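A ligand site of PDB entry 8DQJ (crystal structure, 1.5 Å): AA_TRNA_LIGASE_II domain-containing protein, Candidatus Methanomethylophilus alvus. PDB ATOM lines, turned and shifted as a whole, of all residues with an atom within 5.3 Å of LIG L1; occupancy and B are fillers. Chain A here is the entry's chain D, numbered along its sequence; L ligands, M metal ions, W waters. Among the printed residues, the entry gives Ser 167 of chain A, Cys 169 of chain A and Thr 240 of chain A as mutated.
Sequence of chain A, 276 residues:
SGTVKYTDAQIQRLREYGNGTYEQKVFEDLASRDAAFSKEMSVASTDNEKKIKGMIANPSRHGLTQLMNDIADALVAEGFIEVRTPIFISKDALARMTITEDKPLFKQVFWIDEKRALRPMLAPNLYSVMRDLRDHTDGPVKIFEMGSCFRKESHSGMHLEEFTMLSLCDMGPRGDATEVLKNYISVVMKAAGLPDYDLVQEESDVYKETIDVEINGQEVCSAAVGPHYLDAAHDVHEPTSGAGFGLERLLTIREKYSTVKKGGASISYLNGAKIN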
ATOM      1  N   PRO A 120      -6.591  -0.897 -16.343  1.00  0.00           N
ATOM      2  CA  PRO A 120      -6.045   0.087 -17.295  1.00  0.00           C
ATOM      3  C   PRO A 120      -6.785   0.100 -18.628  1.00  0.00           C
ATOM      4  O   PRO A 120      -6.471   0.908 -19.500  1.00  0.00           O
ATOM      5  CB  PRO A 120      -4.588  -0.375 -17.464  1.00  0.00           C
ATOM      6  CG  PRO A 120      -4.663  -1.855 -17.332  1.00  0.00           C
ATOM      7  CD  PRO A 120      -5.750  -2.118 -16.277  1.00  0.00           C
ATOM      8  N   MET A 121      -7.714  -0.830 -18.808  1.00  0.00           N
ATOM      9  CA  MET A 121      -8.403  -1.119 -20.068  1.00  0.00           C
ATOM     10  C   MET A 121      -9.622  -1.931 -19.697  1.00  0.00           C
ATOM     11  O   MET A 121      -9.651  -2.540 -18.625  1.00  0.00           O
ATOM     12  CB  MET A 121      -7.513  -1.932 -21.042  1.00  0.00           C
ATOM     13  CG  MET A 121      -6.814  -3.216 -20.367  1.00  0.00           C
ATOM     14  SD  MET A 121      -5.674  -4.071 -21.407  1.00  0.00           S
ATOM     15  CE  MET A 121      -6.329  -3.676 -23.040  1.00  0.00           C
ATOM     16  N   LEU A 122     -10.625  -1.925 -20.563  1.00  0.00           N
ATOM     17  CA  LEU A 122     -11.858  -2.681 -20.302  1.00  0.00           C
ATOM     18  C   LEU A 122     -11.818  -4.111 -20.814  1.00  0.00           C
ATOM     19  O   LEU A 122     -12.665  -4.917 -20.403  1.00  0.00           O
ATOM     20  CB  LEU A 122     -13.054  -1.926 -20.962  1.00  0.00           C
ATOM     21  CG  LEU A 122     -13.332  -0.514 -20.440  1.00  0.00           C
ATOM     22  CD1 LEU A 122     -14.474   0.123 -21.196  1.00  0.00           C
ATOM     23  CD2 LEU A 122     -13.660  -0.542 -18.946  1.00  0.00           C
ATOM     24  N   ALA A 123     -10.860  -4.463 -21.652  1.00  0.00           N
ATOM     25  CA  ALA A 123     -10.883  -5.798 -22.253  1.00  0.00           C
ATOM     26  C   ALA A 123     -10.886  -6.941 -21.254  1.00  0.00           C
ATOM     27  O   ALA A 123     -11.573  -7.941 -21.519  1.00  0.00           O
ATOM     28  CB  ALA A 123      -9.680  -5.964 -23.204  1.00  0.00           C
ATOM     29  N   LEU A 126     -14.436  -7.524 -20.150  1.00  0.00           N
ATOM     30  CA  LEU A 126     -15.313  -7.753 -21.293  1.00  0.00           C
ATOM     31  C   LEU A 126     -15.076  -9.133 -21.907  1.00  0.00           C
ATOM     32  O   LEU A 126     -16.016  -9.805 -22.349  1.00  0.00           O
ATOM     33  CB  LEU A 126     -15.152  -6.668 -22.343  1.00  0.00           C
ATOM     34  CG  LEU A 126     -15.671  -5.305 -21.861  1.00  0.00           C
ATOM     35  CD1 LEU A 126     -15.421  -4.269 -22.989  1.00  0.00           C
ATOM     36  CD2 LEU A 126     -17.146  -5.353 -21.513  1.00  0.00           C
ATOM     37  N   TYR A 127     -13.821  -9.589 -21.935  1.00  0.00           N
ATOM     38  CA  TYR A 127     -13.566 -10.950 -22.404  1.00  0.00           C
ATOM     39  C   TYR A 127     -14.317 -11.967 -21.573  1.00  0.00           C
ATOM     40  O   TYR A 127     -14.852 -12.967 -22.113  1.00  0.00           O
ATOM     41  CB  TYR A 127     -12.065 -11.266 -22.340  1.00  0.00           C
ATOM     42  CG  TYR A 127     -11.294 -11.274 -23.645  1.00  0.00           C
ATOM     43  CD1 TYR A 127     -11.602 -12.194 -24.625  1.00  0.00           C
ATOM     44  CD2 TYR A 127     -10.236 -10.418 -23.856  1.00  0.00           C
ATOM     45  CE1 TYR A 127     -10.884 -12.231 -25.830  1.00  0.00           C
ATOM     46  CE2 TYR A 127      -9.509 -10.453 -25.057  1.00  0.00           C
ATOM     47  CZ  TYR A 127      -9.849 -11.358 -26.023  1.00  0.00           C
ATOM     48  OH  TYR A 127      -9.139 -11.434 -27.219  1.00  0.00           O
ATOM     49  N   MET A 130     -18.221 -11.590 -22.282  1.00  0.00           N
ATOM     50  CA  MET A 130     -18.583 -12.064 -23.623  1.00  0.00           C
ATOM     51  C   MET A 130     -18.487 -13.584 -23.695  1.00  0.00           C
ATOM     52  O   MET A 130     -19.382 -14.257 -24.231  1.00  0.00           O
ATOM     53  CB  MET A 130     -17.717 -11.375 -24.694  1.00  0.00           C
ATOM     54  CG  MET A 130     -16.600 -12.084 -25.288  1.00  0.00           C
ATOM     55  SD  MET A 130     -15.894 -11.025 -26.632  1.00  0.00           S
ATOM     56  CE  MET A 130     -17.394 -10.443 -27.416  1.00  0.00           C
ATOM     57  N   ARG A 151      -4.295   4.818 -15.669  1.00  0.00           N
ATOM     58  CA  ARG A 151      -2.908   4.564 -16.029  1.00  0.00           C
ATOM     59  C   ARG A 151      -2.011   5.652 -15.458  1.00  0.00           C
ATOM     60  O   ARG A 151      -2.346   6.830 -15.537  1.00  0.00           O
ATOM     61  CB  ARG A 151      -2.723   4.556 -17.562  1.00  0.00           C
ATOM     62  CG  ARG A 151      -3.481   3.410 -18.240  1.00  0.00           C
ATOM     63  CD  ARG A 151      -3.273   3.410 -19.753  1.00  0.00           C
ATOM     64  NE  ARG A 151      -4.171   2.435 -20.363  1.00  0.00           N
ATOM     65  CZ  ARG A 151      -4.225   2.146 -21.665  1.00  0.00           C
ATOM     66  NH1 ARG A 151      -3.353   2.649 -22.514  1.00  0.00           N
ATOM     67  NH2 ARG A 151      -5.190   1.331 -22.094  1.00  0.00           N
ATOM     68  N   MET A 165     -13.009   4.987 -21.082  1.00  0.00           N
ATOM     69  CA  MET A 165     -12.979   4.166 -22.272  1.00  0.00           C
ATOM     70  C   MET A 165     -14.403   3.759 -22.613  1.00  0.00           C
ATOM     71  O   MET A 165     -15.250   3.534 -21.728  1.00  0.00           O
ATOM     72  CB  MET A 165     -12.084   2.941 -22.035  1.00  0.00           C
ATOM     73  CG  MET A 165     -11.817   2.124 -23.278  1.00  0.00           C
ATOM     74  SD  MET A 165     -10.475   0.892 -23.133  1.00  0.00           S
ATOM     75  CE  MET A 165      -9.282   1.823 -22.232  1.00  0.00           C
ATOM     76  N   SER A 167     -15.499   0.599 -24.759  1.00  0.00           N
ATOM     77  CA  SER A 167     -15.009  -0.568 -25.467  1.00  0.00           C
ATOM     78  C   SER A 167     -16.189  -1.401 -25.909  1.00  0.00           C
ATOM     79  O   SER A 167     -17.107  -1.670 -25.118  1.00  0.00           O
ATOM     80  CB  SER A 167     -14.080  -1.405 -24.612  1.00  0.00           C
ATOM     81  OG  SER A 167     -12.864  -0.691 -24.417  1.00  0.00           O
ATOM     82  N   LEU A 168     -16.166  -1.792 -27.170  1.00  0.00           N
ATOM     83  CA  LEU A 168     -17.163  -2.682 -27.720  1.00  0.00           C
ATOM     84  C   LEU A 168     -16.475  -3.916 -28.229  1.00  0.00           C
ATOM     85  O   LEU A 168     -15.300  -3.896 -28.619  1.00  0.00           O
ATOM     86  CB  LEU A 168     -17.984  -1.975 -28.828  1.00  0.00           C
ATOM     87  CG  LEU A 168     -17.260  -1.528 -30.103  1.00  0.00           C
ATOM     88  CD1 LEU A 168     -17.196  -2.641 -31.068  1.00  0.00           C
ATOM     89  CD2 LEU A 168     -17.999  -0.305 -30.767  1.00  0.00           C
ATOM     90  N   CYS A 169     -17.214  -5.020 -28.249  1.00  0.00           N
ATOM     91  CA  CYS A 169     -16.675  -6.231 -28.808  1.00  0.00           C
ATOM     92  C   CYS A 169     -17.783  -7.115 -29.337  1.00  0.00           C
ATOM     93  O   CYS A 169     -18.932  -7.042 -28.894  1.00  0.00           O
ATOM     94  CB  CYS A 169     -15.778  -6.971 -27.827  1.00  0.00           C
ATOM     95  SG  CYS A 169     -16.327  -7.190 -26.148  1.00  0.00           S
ATOM     96  N   TYR A 207      -1.808  -6.483 -29.128  1.00  0.00           N
ATOM     97  CA  TYR A 207      -2.607  -6.978 -30.244  1.00  0.00           C
ATOM     98  C   TYR A 207      -1.811  -7.236 -31.508  1.00  0.00           C
ATOM     99  O   TYR A 207      -2.395  -7.733 -32.486  1.00  0.00           O
ATOM    100  CB  TYR A 207      -3.724  -5.969 -30.547  1.00  0.00           C
ATOM    101  CG  TYR A 207      -4.698  -5.811 -29.413  1.00  0.00           C
ATOM    102  CD1 TYR A 207      -5.742  -6.702 -29.243  1.00  0.00           C
ATOM    103  CD2 TYR A 207      -4.555  -4.788 -28.498  1.00  0.00           C
ATOM    104  CE1 TYR A 207      -6.635  -6.575 -28.198  1.00  0.00           C
ATOM    105  CE2 TYR A 207      -5.431  -4.648 -27.448  1.00  0.00           C
ATOM    106  CZ  TYR A 207      -6.462  -5.539 -27.306  1.00  0.00           C
ATOM    107  OH  TYR A 207      -7.329  -5.387 -26.255  1.00  0.00           O
ATOM    108  N   THR A 210      -3.104  -2.974 -34.611  1.00  0.00           N
ATOM    109  CA  THR A 210      -4.444  -2.453 -34.426  1.00  0.00           C
ATOM    110  C   THR A 210      -4.810  -1.622 -35.643  1.00  0.00           C
ATOM    111  O   THR A 210      -3.951  -1.231 -36.448  1.00  0.00           O
ATOM    112  CB  THR A 210      -4.555  -1.591 -33.150  1.00  0.00           C
ATOM    113  OG1 THR A 210      -3.606  -0.513 -33.211  1.00  0.00           O
ATOM    114  CG2 THR A 210      -4.283  -2.402 -31.907  1.00  0.00           C
ATOM    115  N   SER A 222      -8.368   2.541 -30.605  1.00  0.00           N
ATOM    116  CA  SER A 222      -7.609   1.404 -31.110  1.00  0.00           C
ATOM    117  C   SER A 222      -8.558   0.222 -31.226  1.00  0.00           C
ATOM    118  O   SER A 222      -9.306  -0.079 -30.286  1.00  0.00           O
ATOM    119  CB  SER A 222      -6.425   1.049 -30.217  1.00  0.00           C
ATOM    120  OG  SER A 222      -5.340   1.953 -30.383  1.00  0.00           O
ATOM    121  N   ALA A 223      -8.515  -0.460 -32.351  1.00  0.00           N
ATOM    122  CA  ALA A 223      -9.411  -1.582 -32.626  1.00  0.00           C
ATOM    123  C   ALA A 223      -8.626  -2.755 -33.175  1.00  0.00           C
ATOM    124  O   ALA A 223      -7.532  -2.601 -33.726  1.00  0.00           O
ATOM    125  CB  ALA A 223     -10.512  -1.177 -33.622  1.00  0.00           C
ATOM    126  N   ALA A 224      -9.167  -3.952 -33.010  1.00  0.00           N
ATOM    127  CA  ALA A 224      -8.485  -5.115 -33.558  1.00  0.00           C
ATOM    128  C   ALA A 224      -9.443  -6.262 -33.785  1.00  0.00           C
ATOM    129  O   ALA A 224     -10.483  -6.377 -33.124  1.00  0.00           O
ATOM    130  CB  ALA A 224      -7.335  -5.578 -32.669  1.00  0.00           C
ATOM    131  N   GLY A 226      -9.240 -10.164 -33.066  1.00  0.00           N
ATOM    132  CA  GLY A 226      -8.400 -11.033 -32.271  1.00  0.00           C
ATOM    133  C   GLY A 226      -7.322 -10.250 -31.546  1.00  0.00           C
ATOM    134  O   GLY A 226      -7.601  -9.216 -30.952  1.00  0.00           O
ATOM    135  N   THR A 240     -13.228 -12.837 -33.043  1.00  0.00           N
ATOM    136  CA  THR A 240     -13.672 -11.745 -32.190  1.00  0.00           C
ATOM    137  C   THR A 240     -13.101 -10.467 -32.758  1.00  0.00           C
ATOM    138  O   THR A 240     -12.056 -10.466 -33.412  1.00  0.00           O
ATOM    139  CB  THR A 240     -13.235 -11.906 -30.730  1.00  0.00           C
ATOM    140  OG1 THR A 240     -11.837 -11.587 -30.609  1.00  0.00           O
ATOM    141  CG2 THR A 240     -13.492 -13.294 -30.241  1.00  0.00           C
ATOM    142  N   SER A 241     -13.793  -9.364 -32.502  1.00  0.00           N
ATOM    143  CA  SER A 241     -13.230  -8.064 -32.798  1.00  0.00           C
ATOM    144  C   SER A 241     -13.619  -7.121 -31.674  1.00  0.00           C
ATOM    145  O   SER A 241     -14.452  -7.428 -30.813  1.00  0.00           O
ATOM    146  CB  SER A 241     -13.688  -7.549 -34.155  1.00  0.00           C
ATOM    147  OG  SER A 241     -15.059  -7.226 -34.141  1.00  0.00           O
ATOM    148  N   GLY A 242     -12.997  -5.967 -31.663  1.00  0.00           N
ATOM    149  CA  GLY A 242     -13.315  -5.018 -30.646  1.00  0.00           C
ATOM    150  C   GLY A 242     -12.654  -3.690 -30.923  1.00  0.00           C
ATOM    151  O   GLY A 242     -11.730  -3.597 -31.733  1.00  0.00           O
ATOM    152  N   ALA A 243     -13.160  -2.670 -30.244  1.00  0.00           N
ATOM    153  CA  ALA A 243     -12.638  -1.312 -30.404  1.00  0.00           C
ATOM    154  C   ALA A 243     -12.708  -0.598 -29.067  1.00  0.00           C
ATOM    155  O   ALA A 243     -13.707  -0.733 -28.343  1.00  0.00           O
ATOM    156  CB  ALA A 243     -13.428  -0.535 -31.461  1.00  0.00           C
ATOM    157  N   GLY A 244     -11.661   0.142 -28.734  1.00  0.00           N
ATOM    158  CA  GLY A 244     -11.642   0.940 -27.522  1.00  0.00           C
ATOM    159  C   GLY A 244     -11.439   2.410 -27.807  1.00  0.00           C
ATOM    160  O   GLY A 244     -10.423   2.776 -28.414  1.00  0.00           O
HETATM  161  C1  LIG L   1     -10.163  -4.773 -28.303  1.00  0.00           C
HETATM  162  C2  LIG L   1     -10.654  -3.996 -27.259  1.00  0.00           C
HETATM  163  C3  LIG L   1     -10.108  -2.746 -27.001  1.00  0.00           C
HETATM  164  C4  LIG L   1      -9.016  -2.374 -27.748  1.00  0.00           C
HETATM  165  C5  LIG L   1      -8.742  -2.981 -28.966  1.00  0.00           C
HETATM  166  C6  LIG L   1      -9.243  -4.224 -29.202  1.00  0.00           C
HETATM  167  C7  LIG L   1      -8.373  -0.985 -27.700  1.00  0.00           C
HETATM  168  C8  LIG L   1      -7.272  -0.822 -26.629  1.00  0.00           C
HETATM  169  C9  LIG L   1      -7.332  -1.481 -25.307  1.00  0.00           C
HETATM  170  C10 LIG L   1     -11.561  -4.602 -26.249  1.00  0.00           C
HETATM  171  C11 LIG L   1     -11.913  -6.068 -26.341  1.00  0.00           C
HETATM  172  C12 LIG L   1     -12.757  -6.636 -25.406  1.00  0.00           C
HETATM  173  C13 LIG L   1     -12.930  -8.026 -25.405  1.00  0.00           C
HETATM  174  C14 LIG L   1     -12.641  -8.742 -26.542  1.00  0.00           C
HETATM  175  C15 LIG L   1     -11.833  -8.168 -27.521  1.00  0.00           C
HETATM  176  C16 LIG L   1     -11.435  -6.844 -27.380  1.00  0.00           C
HETATM  177  N1  LIG L   1     -10.614  -6.190 -28.463  1.00  0.00           N
HETATM  178  N2  LIG L   1      -6.259  -1.469 -27.524  1.00  0.00           N
HETATM  179  O1  LIG L   1     -11.603  -4.046 -25.151  1.00  0.00           O
HETATM  180  O2  LIG L   1      -6.946  -0.744 -24.305  1.00  0.00           O
HETATM  181  O3  LIG L   1      -7.717  -2.664 -25.194  1.00  0.00           O
HETATM  182  P1  LG2 L   2      -1.689   6.531 -26.582  1.00  0.00           P
HETATM  183  O1  LG2 L   2      -0.990   6.626 -25.273  1.00  0.00           O
HETATM  184  O2  LG2 L   2      -2.428   7.782 -27.018  1.00  0.00           O
HETATM  185  O3  LG2 L   2      -0.744   6.042 -27.722  1.00  0.00           O
HETATM  186  P2  LG2 L   2      -2.823   3.840 -26.342  1.00  0.00           P
HETATM  187  O4  LG2 L   2      -2.602   3.166 -27.660  1.00  0.00           O
HETATM  188  O5  LG2 L   2      -1.884   3.544 -25.185  1.00  0.00           O
HETATM  189  O6  LG2 L   2      -2.790   5.383 -26.506  1.00  0.00           O
HETATM  190  P3  LG2 L   2      -5.240   2.201 -25.975  1.00  0.00           P
HETATM  191  O7  LG2 L   2      -4.756   1.122 -25.107  1.00  0.00           O
HETATM  192  O8  LG2 L   2      -5.280   1.889 -27.463  1.00  0.00           O
HETATM  193  O9  LG2 L   2      -4.296   3.488 -25.863  1.00  0.00           O
HETATM  194  O10 LG2 L   2      -6.633   2.698 -25.407  1.00  0.00           O
HETATM  195  C1  LG2 L   2      -7.767   2.901 -26.280  1.00  0.00           C
HETATM  196  C2  LG2 L   2      -8.100   4.367 -26.327  1.00  0.00           C
HETATM  197  O11 LG2 L   2      -8.096   4.874 -24.974  1.00  0.00           O
HETATM  198  C3  LG2 L   2      -6.939   5.136 -26.938  1.00  0.00           C
HETATM  199  O12 LG2 L   2      -7.179   5.150 -28.337  1.00  0.00           O
HETATM  200  C4  LG2 L   2      -7.208   6.549 -26.411  1.00  0.00           C
HETATM  201  O13 LG2 L   2      -8.269   7.147 -27.158  1.00  0.00           O
HETATM  202  C5  LG2 L   2      -7.757   6.262 -25.016  1.00  0.00           C
HETATM  203  N1  LG2 L   2      -6.724   6.456 -24.003  1.00  0.00           N
HETATM  204  C6  LG2 L   2      -5.702   5.597 -23.696  1.00  0.00           C
HETATM  205  N2  LG2 L   2      -4.889   6.031 -22.753  1.00  0.00           N
HETATM  206  C7  LG2 L   2      -5.430   7.259 -22.413  1.00  0.00           C
HETATM  207  C8  LG2 L   2      -5.041   8.244 -21.460  1.00  0.00           C
HETATM  208  N3  LG2 L   2      -4.010   8.110 -20.630  1.00  0.00           N
HETATM  209  N4  LG2 L   2      -5.782   9.366 -21.390  1.00  0.00           N
HETATM  210  C9  LG2 L   2      -6.831   9.505 -22.208  1.00  0.00           C
HETATM  211  N5  LG2 L   2      -7.292   8.658 -23.129  1.00  0.00           N
HETATM  212  C10 LG2 L   2      -6.538   7.552 -23.185  1.00  0.00           C
HETATM  213 MG    MG M   1      -3.914   2.480 -28.946  1.00  0.00          MG
HETATM  214  O   HOH W   1     -10.029  -2.317 -23.615  1.00  0.00           O
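A nitrogen (N2) of LIG L1 lies close to an oxygen (O8) of LG2 L2 (3.5 Å).
Residues that only touch LIG L1: Met 121, Ser 222, Ala 123, Cys 169, Gly 242, Gly 244, Ser 167, Ala 224, Tyr 127, Leu 126, Ala 243, Ala 223 and Met 130.
Hydrophobic or aromatic side chains within 4 Å of LIG L1: Met 121, Ala 123, Leu 126, Tyr 127, Met 130 and Tyr 207.
OG of Ser 167 sits at hydrogen-bond distance from SD of Met 165 (3.1 Å).
O of Ser 222 is in hydrogen-bond range of N of Gly 244, 2.8 Å away.
The backbone NH (N) of Leu 168 is in hydrogen-bond range of the backbone carbonyl oxygen (O) of Ala 243.
The backbone carbonyl oxygen (O) of Pro 120 lies within hydrogen-bond range of the guanidinium group (NE) of Arg 151 (2.9 Å).
The backbone carbonyl oxygen (O) of Gly 242 sits at hydrogen-bond distance from the backbone NH (N) of Ala 224 (2.9 Å).
Water W1 lies within hydrogen-bond range of an oxygen (O1) of LIG L1 (2.8 Å), the backbone NH of Ala 123 (3.0 Å), the backbone NH of Leu 122 (3.1 Å), the side-chain sulfur of Met 165 (3.3 Å) and the side-chain hydroxyl of Ser 167 (3.4 Å).
NH2 of Arg 151 is in salt-bridge range of O7 of LG2 L2 (3.1 Å).
OH of Tyr 207 sits at hydrogen-bond distance from O3 of LIG L1, 2.9 Å away.
O2 of LIG L1 is in salt-bridge range of NH2 of Arg 151 (3.5 Å).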
